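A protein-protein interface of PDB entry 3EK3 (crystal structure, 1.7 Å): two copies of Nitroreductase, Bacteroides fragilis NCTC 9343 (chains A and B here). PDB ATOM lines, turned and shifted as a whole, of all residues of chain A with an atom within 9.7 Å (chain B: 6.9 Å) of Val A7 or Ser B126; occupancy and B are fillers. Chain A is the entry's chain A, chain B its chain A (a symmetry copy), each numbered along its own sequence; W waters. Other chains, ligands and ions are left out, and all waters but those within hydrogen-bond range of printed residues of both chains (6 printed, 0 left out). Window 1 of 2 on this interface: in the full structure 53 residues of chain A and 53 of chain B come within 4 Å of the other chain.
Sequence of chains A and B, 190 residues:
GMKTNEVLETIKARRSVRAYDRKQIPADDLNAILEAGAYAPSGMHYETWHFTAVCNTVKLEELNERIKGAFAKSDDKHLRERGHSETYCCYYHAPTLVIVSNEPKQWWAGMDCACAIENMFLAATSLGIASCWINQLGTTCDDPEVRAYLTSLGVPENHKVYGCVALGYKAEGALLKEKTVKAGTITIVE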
ATOM      1  N   THR A   4       1.331  32.337  29.512  1.00  0.00           N
ATOM      2  CA  THR A   4       1.263  30.853  29.327  1.00  0.00           C
ATOM      3  C   THR A   4       0.032  30.144  29.913  1.00  0.00           C
ATOM      4  O   THR A   4      -0.733  30.717  30.679  1.00  0.00           O
ATOM      5  CB  THR A   4       2.550  30.153  29.841  1.00  0.00           C
ATOM      6  OG1 THR A   4       2.624  28.855  29.247  1.00  0.00           O
ATOM      7  CG2 THR A   4       2.579  30.031  31.343  1.00  0.00           C
ATOM      8  N   ASN A   5      -0.142  28.885  29.525  1.00  0.00           N
ATOM      9  CA  ASN A   5      -1.181  28.021  30.071  1.00  0.00           C
ATOM     10  C   ASN A   5      -0.822  26.560  29.786  1.00  0.00           C
ATOM     11  O   ASN A   5       0.205  26.305  29.195  1.00  0.00           O
ATOM     12  CB  ASN A   5      -2.561  28.428  29.557  1.00  0.00           C
ATOM     13  CG  ASN A   5      -2.713  28.243  28.080  1.00  0.00           C
ATOM     14  OD1 ASN A   5      -2.259  27.248  27.531  1.00  0.00           O
ATOM     15  ND2 ASN A   5      -3.359  29.200  27.430  1.00  0.00           N
ATOM     16  N   GLU A   6      -1.610  25.605  30.249  1.00  0.00           N
ATOM     17  CA  GLU A   6      -1.211  24.203  30.106  1.00  0.00           C
ATOM     18  C   GLU A   6      -1.125  23.814  28.637  1.00  0.00           C
ATOM     19  O   GLU A   6      -0.227  23.061  28.274  1.00  0.00           O
ATOM     20  CB  GLU A   6      -2.177  23.266  30.793  1.00  0.00           C
ATOM     21  CG  GLU A   6      -2.072  23.350  32.296  1.00  0.00           C
ATOM     22  CD  GLU A   6      -2.842  22.280  33.043  1.00  0.00           C
ATOM     23  OE1 GLU A   6      -3.472  21.399  32.413  1.00  0.00           O
ATOM     24  OE2 GLU A   6      -2.802  22.337  34.289  1.00  0.00           O
ATOM     25  N   VAL A   7      -2.025  24.330  27.813  1.00  0.00           N
ATOM     26  CA  VAL A   7      -1.977  23.999  26.378  1.00  0.00           C
ATOM     27  C   VAL A   7      -0.689  24.506  25.725  1.00  0.00           C
ATOM     28  O   VAL A   7       0.013  23.767  25.024  1.00  0.00           O
ATOM     29  CB  VAL A   7      -3.198  24.550  25.597  1.00  0.00           C
ATOM     30  CG1 VAL A   7      -3.021  24.363  24.071  1.00  0.00           C
ATOM     31  CG2 VAL A   7      -4.475  23.839  26.060  1.00  0.00           C
ATOM     32  N   LEU A   8      -0.388  25.772  25.953  1.00  0.00           N
ATOM     33  CA  LEU A   8       0.807  26.377  25.402  1.00  0.00           C
ATOM     34  C   LEU A   8       2.063  25.659  25.868  1.00  0.00           C
ATOM     35  O   LEU A   8       2.989  25.433  25.085  1.00  0.00           O
ATOM     36  CB  LEU A   8       0.827  27.845  25.758  1.00  0.00           C
ATOM     37  CG  LEU A   8      -0.310  28.715  25.182  1.00  0.00           C
ATOM     38  CD1 LEU A   8      -0.195  30.139  25.634  1.00  0.00           C
ATOM     39  CD2 LEU A   8      -0.305  28.643  23.634  1.00  0.00           C
ATOM     40  N   GLU A   9       2.105  25.298  27.145  1.00  0.00           N
ATOM     41  CA  GLU A   9       3.270  24.602  27.671  1.00  0.00           C
ATOM     42  C   GLU A   9       3.385  23.186  27.104  1.00  0.00           C
ATOM     43  O   GLU A   9       4.502  22.722  26.849  1.00  0.00           O
ATOM     44  CB  GLU A   9       3.289  24.610  29.200  1.00  0.00           C
ATOM     45  CG  GLU A   9       3.554  26.005  29.783  1.00  0.00           C
ATOM     46  CD  GLU A   9       4.840  26.654  29.251  1.00  0.00           C
ATOM     47  OE1 GLU A   9       5.923  26.050  29.369  1.00  0.00           O
ATOM     48  OE2 GLU A   9       4.762  27.772  28.714  1.00  0.00           O
ATOM     49  N   THR A  10       2.256  22.521  26.884  1.00  0.00           N
ATOM     50  CA  THR A  10       2.258  21.161  26.355  1.00  0.00           C
ATOM     51  C   THR A  10       2.731  21.218  24.916  1.00  0.00           C
ATOM     52  O   THR A  10       3.528  20.412  24.502  1.00  0.00           O
ATOM     53  CB  THR A  10       0.866  20.518  26.422  1.00  0.00           C
ATOM     54  OG1 THR A  10       0.431  20.482  27.804  1.00  0.00           O
ATOM     55  CG2 THR A  10       0.868  19.110  25.844  1.00  0.00           C
ATOM     56  N   ILE A  11       2.305  22.246  24.208  1.00  0.00           N
ATOM     57  CA  ILE A  11       2.746  22.428  22.818  1.00  0.00           C
ATOM     58  C   ILE A  11       4.283  22.586  22.734  1.00  0.00           C
ATOM     59  O   ILE A  11       4.930  21.959  21.888  1.00  0.00           O
ATOM     60  CB  ILE A  11       2.029  23.630  22.164  1.00  0.00           C
ATOM     61  CG1 ILE A  11       0.590  23.223  21.770  1.00  0.00           C
ATOM     62  CG2 ILE A  11       2.794  24.132  20.946  1.00  0.00           C
ATOM     63  CD1 ILE A  11      -0.338  24.382  21.350  1.00  0.00           C
ATOM     64  N   LYS A  12       4.863  23.438  23.569  1.00  0.00           N
ATOM     65  CA  LYS A  12       6.322  23.582  23.634  1.00  0.00           C
ATOM     66  C   LYS A  12       7.038  22.336  24.131  1.00  0.00           C
ATOM     67  O   LYS A  12       8.177  22.097  23.738  1.00  0.00           O
ATOM     68  CB  LYS A  12       6.716  24.773  24.501  1.00  0.00           C
ATOM     69  CG  LYS A  12       6.357  26.118  23.926  1.00  0.00           C
ATOM     70  CD  LYS A  12       6.516  27.153  25.041  1.00  0.00           C
ATOM     71  CE  LYS A  12       6.716  28.529  24.538  1.00  0.00           C
ATOM     72  NZ  LYS A  12       7.034  29.470  25.676  1.00  0.00           N
ATOM     73  N   ALA A  13       6.389  21.547  24.986  1.00  0.00           N
ATOM     74  CA  ALA A  13       7.038  20.391  25.619  1.00  0.00           C
ATOM     75  C   ALA A  13       7.023  19.146  24.736  1.00  0.00           C
ATOM     76  O   ALA A  13       7.828  18.237  24.951  1.00  0.00           O
ATOM     77  CB  ALA A  13       6.400  20.078  26.959  1.00  0.00           C
ATOM     78  N   ARG A  14       6.123  19.101  23.764  1.00  0.00           N
ATOM     79  CA  ARG A  14       6.030  17.963  22.836  1.00  0.00           C
ATOM     80  C   ARG A  14       7.331  17.755  22.087  1.00  0.00           C
ATOM     81  O   ARG A  14       7.819  18.664  21.400  1.00  0.00           O
ATOM     82  CB  ARG A  14       4.890  18.151  21.840  1.00  0.00           C
ATOM     83  CG  ARG A  14       4.677  16.974  20.894  1.00  0.00           C
ATOM     84  CD  ARG A  14       4.363  17.391  19.469  1.00  0.00           C
ATOM     85  NE  ARG A  14       5.304  18.379  18.967  1.00  0.00           N
ATOM     86  CZ  ARG A  14       6.528  18.103  18.526  1.00  0.00           C
ATOM     87  NH1 ARG A  14       6.977  16.867  18.489  1.00  0.00           N
ATOM     88  NH2 ARG A  14       7.312  19.090  18.156  1.00  0.00           N
ATOM     89  N   GLU A 118      -1.052  15.633  14.938  1.00  0.00           N
ATOM     90  CA  GLU A 118      -0.616  16.650  15.889  1.00  0.00           C
ATOM     91  C   GLU A 118      -1.467  16.624  17.153  1.00  0.00           C
ATOM     92  O   GLU A 118      -0.905  16.679  18.238  1.00  0.00           O
ATOM     93  CB  GLU A 118      -0.555  18.030  15.246  1.00  0.00           C
ATOM     94  CG  GLU A 118       0.062  19.163  16.074  1.00  0.00           C
ATOM     95  CD  GLU A 118       1.511  18.922  16.478  1.00  0.00           C
ATOM     96  OE1 GLU A 118       2.126  18.040  15.906  1.00  0.00           O
ATOM     97  OE2 GLU A 118       2.052  19.596  17.399  1.00  0.00           O
ATOM     98  N   ASN A 119      -2.780  16.494  17.023  1.00  0.00           N
ATOM     99  CA  ASN A 119      -3.639  16.316  18.213  1.00  0.00           C
ATOM    100  C   ASN A 119      -3.206  15.134  19.096  1.00  0.00           C
ATOM    101  O   ASN A 119      -3.164  15.228  20.315  1.00  0.00           O
ATOM    102  CB  ASN A 119      -5.117  16.148  17.784  1.00  0.00           C
ATOM    103  CG  ASN A 119      -5.778  17.465  17.471  1.00  0.00           C
ATOM    104  OD1 ASN A 119      -5.129  18.525  17.505  1.00  0.00           O
ATOM    105  ND2 ASN A 119      -7.091  17.418  17.178  1.00  0.00           N
ATOM    106  N   LEU A 122      -0.032  15.824  21.051  1.00  0.00           N
ATOM    107  CA  LEU A 122      -0.327  16.729  22.157  1.00  0.00           C
ATOM    108  C   LEU A 122      -1.136  16.051  23.263  1.00  0.00           C
ATOM    109  O   LEU A 122      -0.841  16.192  24.453  1.00  0.00           O
ATOM    110  CB  LEU A 122      -1.023  17.980  21.616  1.00  0.00           C
ATOM    111  CG  LEU A 122      -0.164  18.854  20.692  1.00  0.00           C
ATOM    112  CD1 LEU A 122      -0.981  20.038  20.090  1.00  0.00           C
ATOM    113  CD2 LEU A 122       1.117  19.372  21.371  1.00  0.00           C
ATOM    114  N   ALA A 123      -2.132  15.274  22.862  1.00  0.00           N
ATOM    115  CA  ALA A 123      -2.875  14.441  23.792  1.00  0.00           C
ATOM    116  C   ALA A 123      -1.894  13.523  24.560  1.00  0.00           C
ATOM    117  O   ALA A 123      -1.964  13.408  25.777  1.00  0.00           O
ATOM    118  CB  ALA A 123      -3.907  13.630  23.034  1.00  0.00           C
ATOM    119  N   THR A 125       1.379  13.828  25.002  1.00  0.00           N
ATOM    120  CA  THR A 125       2.253  14.606  25.881  1.00  0.00           C
ATOM    121  C   THR A 125       1.507  14.981  27.146  1.00  0.00           C
ATOM    122  O   THR A 125       2.068  14.894  28.240  1.00  0.00           O
ATOM    123  CB  THR A 125       2.804  15.854  25.172  1.00  0.00           C
ATOM    124  OG1 THR A 125       3.568  15.467  24.031  1.00  0.00           O
ATOM    125  CG2 THR A 125       3.710  16.650  26.120  1.00  0.00           C
ATOM    126  N   SER A 126       0.246  15.391  27.012  1.00  0.00           N
ATOM    127  CA  SER A 126      -0.524  15.813  28.209  1.00  0.00           C
ATOM    128  C   SER A 126      -0.762  14.681  29.196  1.00  0.00           C
ATOM    129  O   SER A 126      -1.074  14.947  30.352  1.00  0.00           O
ATOM    130  CB  SER A 126      -1.871  16.418  27.819  1.00  0.00           C
ATOM    131  OG  SER A 126      -2.790  15.396  27.499  1.00  0.00           O
ATOM    132  N   GLU B   6      -6.825  19.751  30.605  1.00  0.00           N
ATOM    133  CA  GLU B   6      -7.085  20.975  29.845  1.00  0.00           C
ATOM    134  C   GLU B   6      -6.724  20.786  28.379  1.00  0.00           C
ATOM    135  O   GLU B   6      -7.435  21.299  27.520  1.00  0.00           O
ATOM    136  CB  GLU B   6      -6.306  22.153  30.382  1.00  0.00           C
ATOM    137  CG  GLU B   6      -6.844  22.626  31.710  1.00  0.00           C
ATOM    138  CD  GLU B   6      -6.261  23.938  32.194  1.00  0.00           C
ATOM    139  OE1 GLU B   6      -5.429  24.556  31.493  1.00  0.00           O
ATOM    140  OE2 GLU B   6      -6.661  24.345  33.304  1.00  0.00           O
ATOM    141  N   VAL B   7      -5.656  20.053  28.101  1.00  0.00           N
ATOM    142  CA  VAL B   7      -5.270  19.825  26.697  1.00  0.00           C
ATOM    143  C   VAL B   7      -6.343  19.040  25.937  1.00  0.00           C
ATOM    144  O   VAL B   7      -6.771  19.426  24.843  1.00  0.00           O
ATOM    145  CB  VAL B   7      -3.910  19.094  26.562  1.00  0.00           C
ATOM    146  CG1 VAL B   7      -3.630  18.692  25.095  1.00  0.00           C
ATOM    147  CG2 VAL B   7      -2.782  19.997  27.075  1.00  0.00           C
ATOM    148  N   LEU B   8      -6.768  17.934  26.522  1.00  0.00           N
ATOM    149  CA  LEU B   8      -7.786  17.101  25.916  1.00  0.00           C
ATOM    150  C   LEU B   8      -9.081  17.869  25.700  1.00  0.00           C
ATOM    151  O   LEU B   8      -9.728  17.736  24.659  1.00  0.00           O
ATOM    152  CB  LEU B   8      -7.991  15.871  26.769  1.00  0.00           C
ATOM    153  CG  LEU B   8      -6.787  14.916  26.909  1.00  0.00           C
ATOM    154  CD1 LEU B   8      -7.107  13.757  27.803  1.00  0.00           C
ATOM    155  CD2 LEU B   8      -6.343  14.409  25.514  1.00  0.00           C
ATOM    156  N   THR B  10      -9.380  21.144  25.379  1.00  0.00           N
ATOM    157  CA  THR B  10      -9.152  22.208  24.407  1.00  0.00           C
ATOM    158  C   THR B  10      -9.194  21.596  23.021  1.00  0.00           C
ATOM    159  O   THR B  10      -9.792  22.144  22.128  1.00  0.00           O
ATOM    160  CB  THR B  10      -7.804  22.908  24.628  1.00  0.00           C
ATOM    161  OG1 THR B  10      -7.783  23.478  25.960  1.00  0.00           O
ATOM    162  CG2 THR B  10      -7.560  23.999  23.595  1.00  0.00           C
ATOM    163  N   ILE B  11      -8.641  20.404  22.899  1.00  0.00           N
ATOM    164  CA  ILE B  11      -8.674  19.695  21.613  1.00  0.00           C
ATOM    165  C   ILE B  11     -10.128  19.431  21.155  1.00  0.00           C
ATOM    166  O   ILE B  11     -10.468  19.661  19.990  1.00  0.00           O
ATOM    167  CB  ILE B  11      -7.868  18.378  21.687  1.00  0.00           C
ATOM    168  CG1 ILE B  11      -6.356  18.692  21.601  1.00  0.00           C
ATOM    169  CG2 ILE B  11      -8.278  17.419  20.577  1.00  0.00           C
ATOM    170  CD1 ILE B  11      -5.414  17.513  21.926  1.00  0.00           C
ATOM    171  N   ALA B  36       3.467  28.860  19.028  1.00  0.00           N
ATOM    172  CA  ALA B  36       2.934  27.497  19.121  1.00  0.00           C
ATOM    173  C   ALA B  36       3.093  26.791  17.772  1.00  0.00           C
ATOM    174  O   ALA B  36       3.530  25.649  17.753  1.00  0.00           O
ATOM    175  CB  ALA B  36       1.473  27.487  19.598  1.00  0.00           C
ATOM    176  N   ASN B 119      -1.389  23.361  15.884  1.00  0.00           N
ATOM    177  CA  ASN B 119      -0.899  24.015  17.116  1.00  0.00           C
ATOM    178  C   ASN B 119      -1.500  25.415  17.333  1.00  0.00           C
ATOM    179  O   ASN B 119      -1.896  25.777  18.433  1.00  0.00           O
ATOM    180  CB  ASN B 119       0.647  24.096  17.100  1.00  0.00           C
ATOM    181  CG  ASN B 119       1.295  22.797  17.501  1.00  0.00           C
ATOM    182  OD1 ASN B 119       0.604  21.790  17.738  1.00  0.00           O
ATOM    183  ND2 ASN B 119       2.636  22.806  17.603  1.00  0.00           N
ATOM    184  N   MET B 120      -1.518  26.204  16.275  1.00  0.00           N
ATOM    185  CA  MET B 120      -2.036  27.563  16.315  1.00  0.00           C
ATOM    186  C   MET B 120      -3.516  27.588  16.691  1.00  0.00           C
ATOM    187  O   MET B 120      -3.919  28.374  17.560  1.00  0.00           O
ATOM    188  CB  MET B 120      -1.824  28.228  14.953  1.00  0.00           C
ATOM    189  CG  MET B 120      -0.401  28.581  14.696  1.00  0.00           C
ATOM    190  SD  MET B 120      -0.289  29.792  13.138  1.00  0.00           S
ATOM    191  CE  MET B 120       1.598  29.548  12.757  1.00  0.00           C
ATOM    192  N   PHE B 121      -4.311  26.696  16.086  1.00  0.00           N
ATOM    193  CA  PHE B 121      -5.746  26.553  16.431  1.00  0.00           C
ATOM    194  C   PHE B 121      -5.924  26.283  17.919  1.00  0.00           C
ATOM    195  O   PHE B 121      -6.751  26.889  18.607  1.00  0.00           O
ATOM    196  CB  PHE B 121      -6.427  25.406  15.698  1.00  0.00           C
ATOM    197  CG  PHE B 121      -6.574  25.586  14.182  1.00  0.00           C
ATOM    198  CD1 PHE B 121      -6.675  26.850  13.560  1.00  0.00           C
ATOM    199  CD2 PHE B 121      -6.713  24.455  13.392  1.00  0.00           C
ATOM    200  CE1 PHE B 121      -6.841  26.944  12.153  1.00  0.00           C
ATOM    201  CE2 PHE B 121      -6.902  24.537  12.000  1.00  0.00           C
ATOM    202  CZ  PHE B 121      -6.963  25.797  11.390  1.00  0.00           C
ATOM    203  N   LEU B 122      -5.136  25.320  18.403  1.00  0.00           N
ATOM    204  CA  LEU B 122      -5.223  24.907  19.800  1.00  0.00           C
ATOM    205  C   LEU B 122      -4.729  25.991  20.758  1.00  0.00           C
ATOM    206  O   LEU B 122      -5.361  26.286  21.777  1.00  0.00           O
ATOM    207  CB  LEU B 122      -4.473  23.586  19.986  1.00  0.00           C
ATOM    208  CG  LEU B 122      -5.078  22.385  19.246  1.00  0.00           C
ATOM    209  CD1 LEU B 122      -4.191  21.110  19.388  1.00  0.00           C
ATOM    210  CD2 LEU B 122      -6.527  22.084  19.671  1.00  0.00           C
ATOM    211  N   ALA B 123      -3.618  26.619  20.402  1.00  0.00           N
ATOM    212  CA  ALA B 123      -3.127  27.778  21.128  1.00  0.00           C
ATOM    213  C   ALA B 123      -4.234  28.858  21.185  1.00  0.00           C
ATOM    214  O   ALA B 123      -4.510  29.421  22.237  1.00  0.00           O
ATOM    215  CB  ALA B 123      -1.877  28.307  20.455  1.00  0.00           C
ATOM    216  N   ALA B 124      -4.833  29.158  20.039  1.00  0.00           N
ATOM    217  CA  ALA B 124      -5.880  30.183  19.964  1.00  0.00           C
ATOM    218  C   ALA B 124      -7.051  29.803  20.846  1.00  0.00           C
ATOM    219  O   ALA B 124      -7.528  30.611  21.634  1.00  0.00           O
ATOM    220  CB  ALA B 124      -6.331  30.371  18.538  1.00  0.00           C
ATOM    221  N   THR B 125      -7.508  28.554  20.747  1.00  0.00           N
ATOM    222  CA  THR B 125      -8.640  28.110  21.560  1.00  0.00           C
ATOM    223  C   THR B 125      -8.312  28.273  23.031  1.00  0.00           C
ATOM    224  O   THR B 125      -9.158  28.728  23.804  1.00  0.00           O
ATOM    225  CB  THR B 125      -9.033  26.658  21.238  1.00  0.00           C
ATOM    226  OG1 THR B 125      -9.414  26.552  19.868  1.00  0.00           O
ATOM    227  CG2 THR B 125     -10.218  26.221  22.111  1.00  0.00           C
ATOM    228  N   SER B 126      -7.091  27.915  23.427  1.00  0.00           N
ATOM    229  CA  SER B 126      -6.722  28.010  24.862  1.00  0.00           C
ATOM    230  C   SER B 126      -6.715  29.439  25.383  1.00  0.00           C
ATOM    231  O   SER B 126      -6.764  29.639  26.592  1.00  0.00           O
ATOM    232  CB  SER B 126      -5.357  27.381  25.129  1.00  0.00           C
ATOM    233  OG  SER B 126      -4.328  28.263  24.732  1.00  0.00           O
ATOM    234  N   LEU B 127      -6.688  30.413  24.480  1.00  0.00           N
ATOM    235  CA  LEU B 127      -6.676  31.838  24.804  1.00  0.00           C
ATOM    236  C   LEU B 127      -8.011  32.559  24.549  1.00  0.00           C
ATOM    237  O   LEU B 127      -8.091  33.798  24.622  1.00  0.00           O
ATOM    238  CB  LEU B 127      -5.564  32.494  24.006  1.00  0.00           C
ATOM    239  CG  LEU B 127      -4.137  32.043  24.354  1.00  0.00           C
ATOM    240  CD1 LEU B 127      -3.158  32.475  23.241  1.00  0.00           C
ATOM    241  CD2 LEU B 127      -3.673  32.567  25.686  1.00  0.00           C
ATOM    242  N   GLY B 128      -9.056  31.785  24.265  1.00  0.00           N
ATOM    243  CA  GLY B 128     -10.369  32.328  23.905  1.00  0.00           C
ATOM    244  C   GLY B 128     -10.517  33.001  22.557  1.00  0.00           C
ATOM    245  O   GLY B 128     -11.467  33.750  22.328  1.00  0.00           O
ATOM    246  N   ILE B 129      -9.582  32.682  21.673  1.00  0.00           N
ATOM    247  CA  ILE B 129      -9.500  33.239  20.332  1.00  0.00           C
ATOM    248  C   ILE B 129     -10.009  32.215  19.319  1.00  0.00           C
ATOM    249  O   ILE B 129      -9.517  31.083  19.273  1.00  0.00           O
ATOM    250  CB  ILE B 129      -8.043  33.655  20.044  1.00  0.00           C
ATOM    251  CG1 ILE B 129      -7.713  34.930  20.822  1.00  0.00           C
ATOM    252  CG2 ILE B 129      -7.802  33.822  18.525  1.00  0.00           C
ATOM    253  CD1 ILE B 129      -6.229  35.265  20.890  1.00  0.00           C
HETATM  254  O   HOH W   1      -5.483  19.837  33.281  1.00  0.00           O
HETATM  255  O   HOH W   2       4.632  21.221  19.383  1.00  0.00           O
HETATM  256  O   HOH W   3      -9.421  19.434  17.589  1.00  0.00           O
HETATM  257  O   HOH W   4      -3.667  26.440  32.259  1.00  0.00           O
HETATM  258  O   HOH W   5      -3.474  19.569  30.350  1.00  0.00           O
HETATM  259  O   HOH W   6      -4.730  25.489  28.993  1.00  0.00           O
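Val A7 touches Thr B10, and with the chains exchanged Thr A10 touches Val B7.
Val A7 touches Leu B122, and with the chains exchanged Leu A122 touches Val B7.
Val A7 touches Ser B126, and with the chains exchanged Ser A126 touches Val B7.
Ile A11 touches Asn B119, and with the chains exchanged Asn A119 touches Ile B11.
Thr A4 touches none of the printed residues of chain B.
Printed residues of chain B within 4 Å of Asn A5: Ser B126 and Leu B127.
Of the printed residues of chain B, Glu A6 touches Glu B6.
Of chain B, only Thr B10, Leu B122 and Ser B126 come within 4 Å of Val A7.
Of the printed residues of chain B, Ala A123 touches Leu B8 (3.6 Å).
Of the printed residues of chain B, Ser A126 touches Val B7 (3.6 Å).
Val B7 touches just these residues of chain A: Thr A10 (3.3 Å), Leu A122 (3.8 Å) and Ser A126 (3.6 Å).
Of the printed residues of chain A, Asn B119 touches Ile A11, Glu A118 and Leu A122.
Ala B123 touches just one residue of chain A: Leu A8 (3.6 Å).
Ala B124 touches none of the printed residues of chain A.
No residue of chain A comes within 4 Å of Thr B125.
Ser B126 touches two residues of chain A.
Leu B127 touches one residue of chain A.
The nearest printed residue of chain B that does not touch Thr A10 is Glu B6 (7.2 Å).
Hydrophobic or aromatic side chains of chain B that line the printed part of chain A: Val B7, Leu B8, Ile B11, Ala B36, Leu B122, Ala B123 and Leu B127.
Of the 17 printed residues of chain A, 11 touch a printed residue of chain B.
Printed residues of chain A that touch a printed residue of chain B: Asn A5, Glu A6, Val A7, Leu A8, Thr A10, Ile A11, Glu A118, Asn A119, Leu A122, Ala A123 and Ser A126.
Hydrophobic or aromatic side chains of chain A within 4 Å of the printed part of chain B: Val A7, Leu A8, Ile A11, Leu A122 and Ala A123.
Among the printed residues, 18 pairs touch across the chains.
Among the printed residues, no Asp or Glu carboxylate lies within 4 Å of a Lys or Arg side-chain nitrogen of the other chain.
The side-chain hydroxyl of Ser B126 is in hydrogen-bond range of the side-chain amide nitrogen of Asn A5 (3.0 Å).
The side-chain amide oxygen (OD1) of Asn B119 lies close to the side-chain carboxylate (OE2) of Glu A118 (2.7 Å).
Water W3 lies within hydrogen-bond range of the backbone carbonyl oxygen (O) of Ile B11 (2.6 Å) and the side-chain amide nitrogen (ND2) of Asn A119 (3.1 Å).
Water W2 lies within hydrogen-bond range of the backbone carbonyl oxygen of Ile A11 (2.6 Å), the guanidinium group of Arg A14 (2.9 Å) and the side-chain amide nitrogen of Asn B119 (3.1 Å).
Water W1 bridges the side-chain carboxylate of Glu A6 (2.7 Å) and the backbone NH of Glu B6 (3.0 Å).
Water W4 lies within hydrogen-bond range of OE1 of Glu B6 (2.7 Å) and N of Glu A6 (3.0 Å).
Water W5 lies within hydrogen-bond range of OE1 of Glu A6 (2.8 Å), N of Val B7 (3.2 Å) and N of Glu B6 (3.4 Å).
Water W6 lies within hydrogen-bond range of the side-chain carboxylate of Glu B6 (2.8 Å), the backbone NH of Val A7 (3.2 Å), the backbone NH of Glu A6 (3.4 Å) and the side-chain amide oxygen of Asn A5 (3.4 Å).
Among the printed residues, pairs that only touch across the chains: Val A7 with Thr B10 (3.3 Å), Thr A10 with Val B7 (3.3 Å), Asn A119 with Leu B122 (3.3 Å), Leu A122 with Asn B119 (3.3 Å), Leu A122 with Leu B122 (3.5 Å), Leu A8 with Ala B123 (3.6 Å), Ala A123 with Leu B8 (3.6 Å), Glu A6 with Glu B6 (3.6 Å), Asn A119 with Ile B11 (3.6 Å), Ile A11 with Asn B119 (3.6 Å), Val A7 with Ser B126 (3.6 Å), Ser A126 with Val B7 (3.6 Å), Ile A11 with Ala B36 (3.6 Å), Val A7 with Leu B122 (3.8 Å), Leu A122 with Val B7 (3.8 Å) and Asn A5 with Leu B127 (3.8 Å).
OD1 of Asn A5 lies within hydrogen-bond range of N of Val A7, at 2.9 Å.
The side-chain amide oxygen (OD1) of Asn A5 lies within hydrogen-bond range of the backbone NH (N) of Leu A8.
The side-chain hydroxyl (OG1) of Thr A10 sits at hydrogen-bond distance from the backbone carbonyl oxygen (O) of Glu A6 (2.7 Å).
O of Ala A123 lies within hydrogen-bond range of OG of Ser A126 (2.8 Å).
The backbone carbonyl oxygen (O) of Glu B6 lies within hydrogen-bond range of the side-chain hydroxyl (OG1) of Thr B10.
O of Ala B36 sits at hydrogen-bond distance from ND2 of Asn B119, at 3.0 Å.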
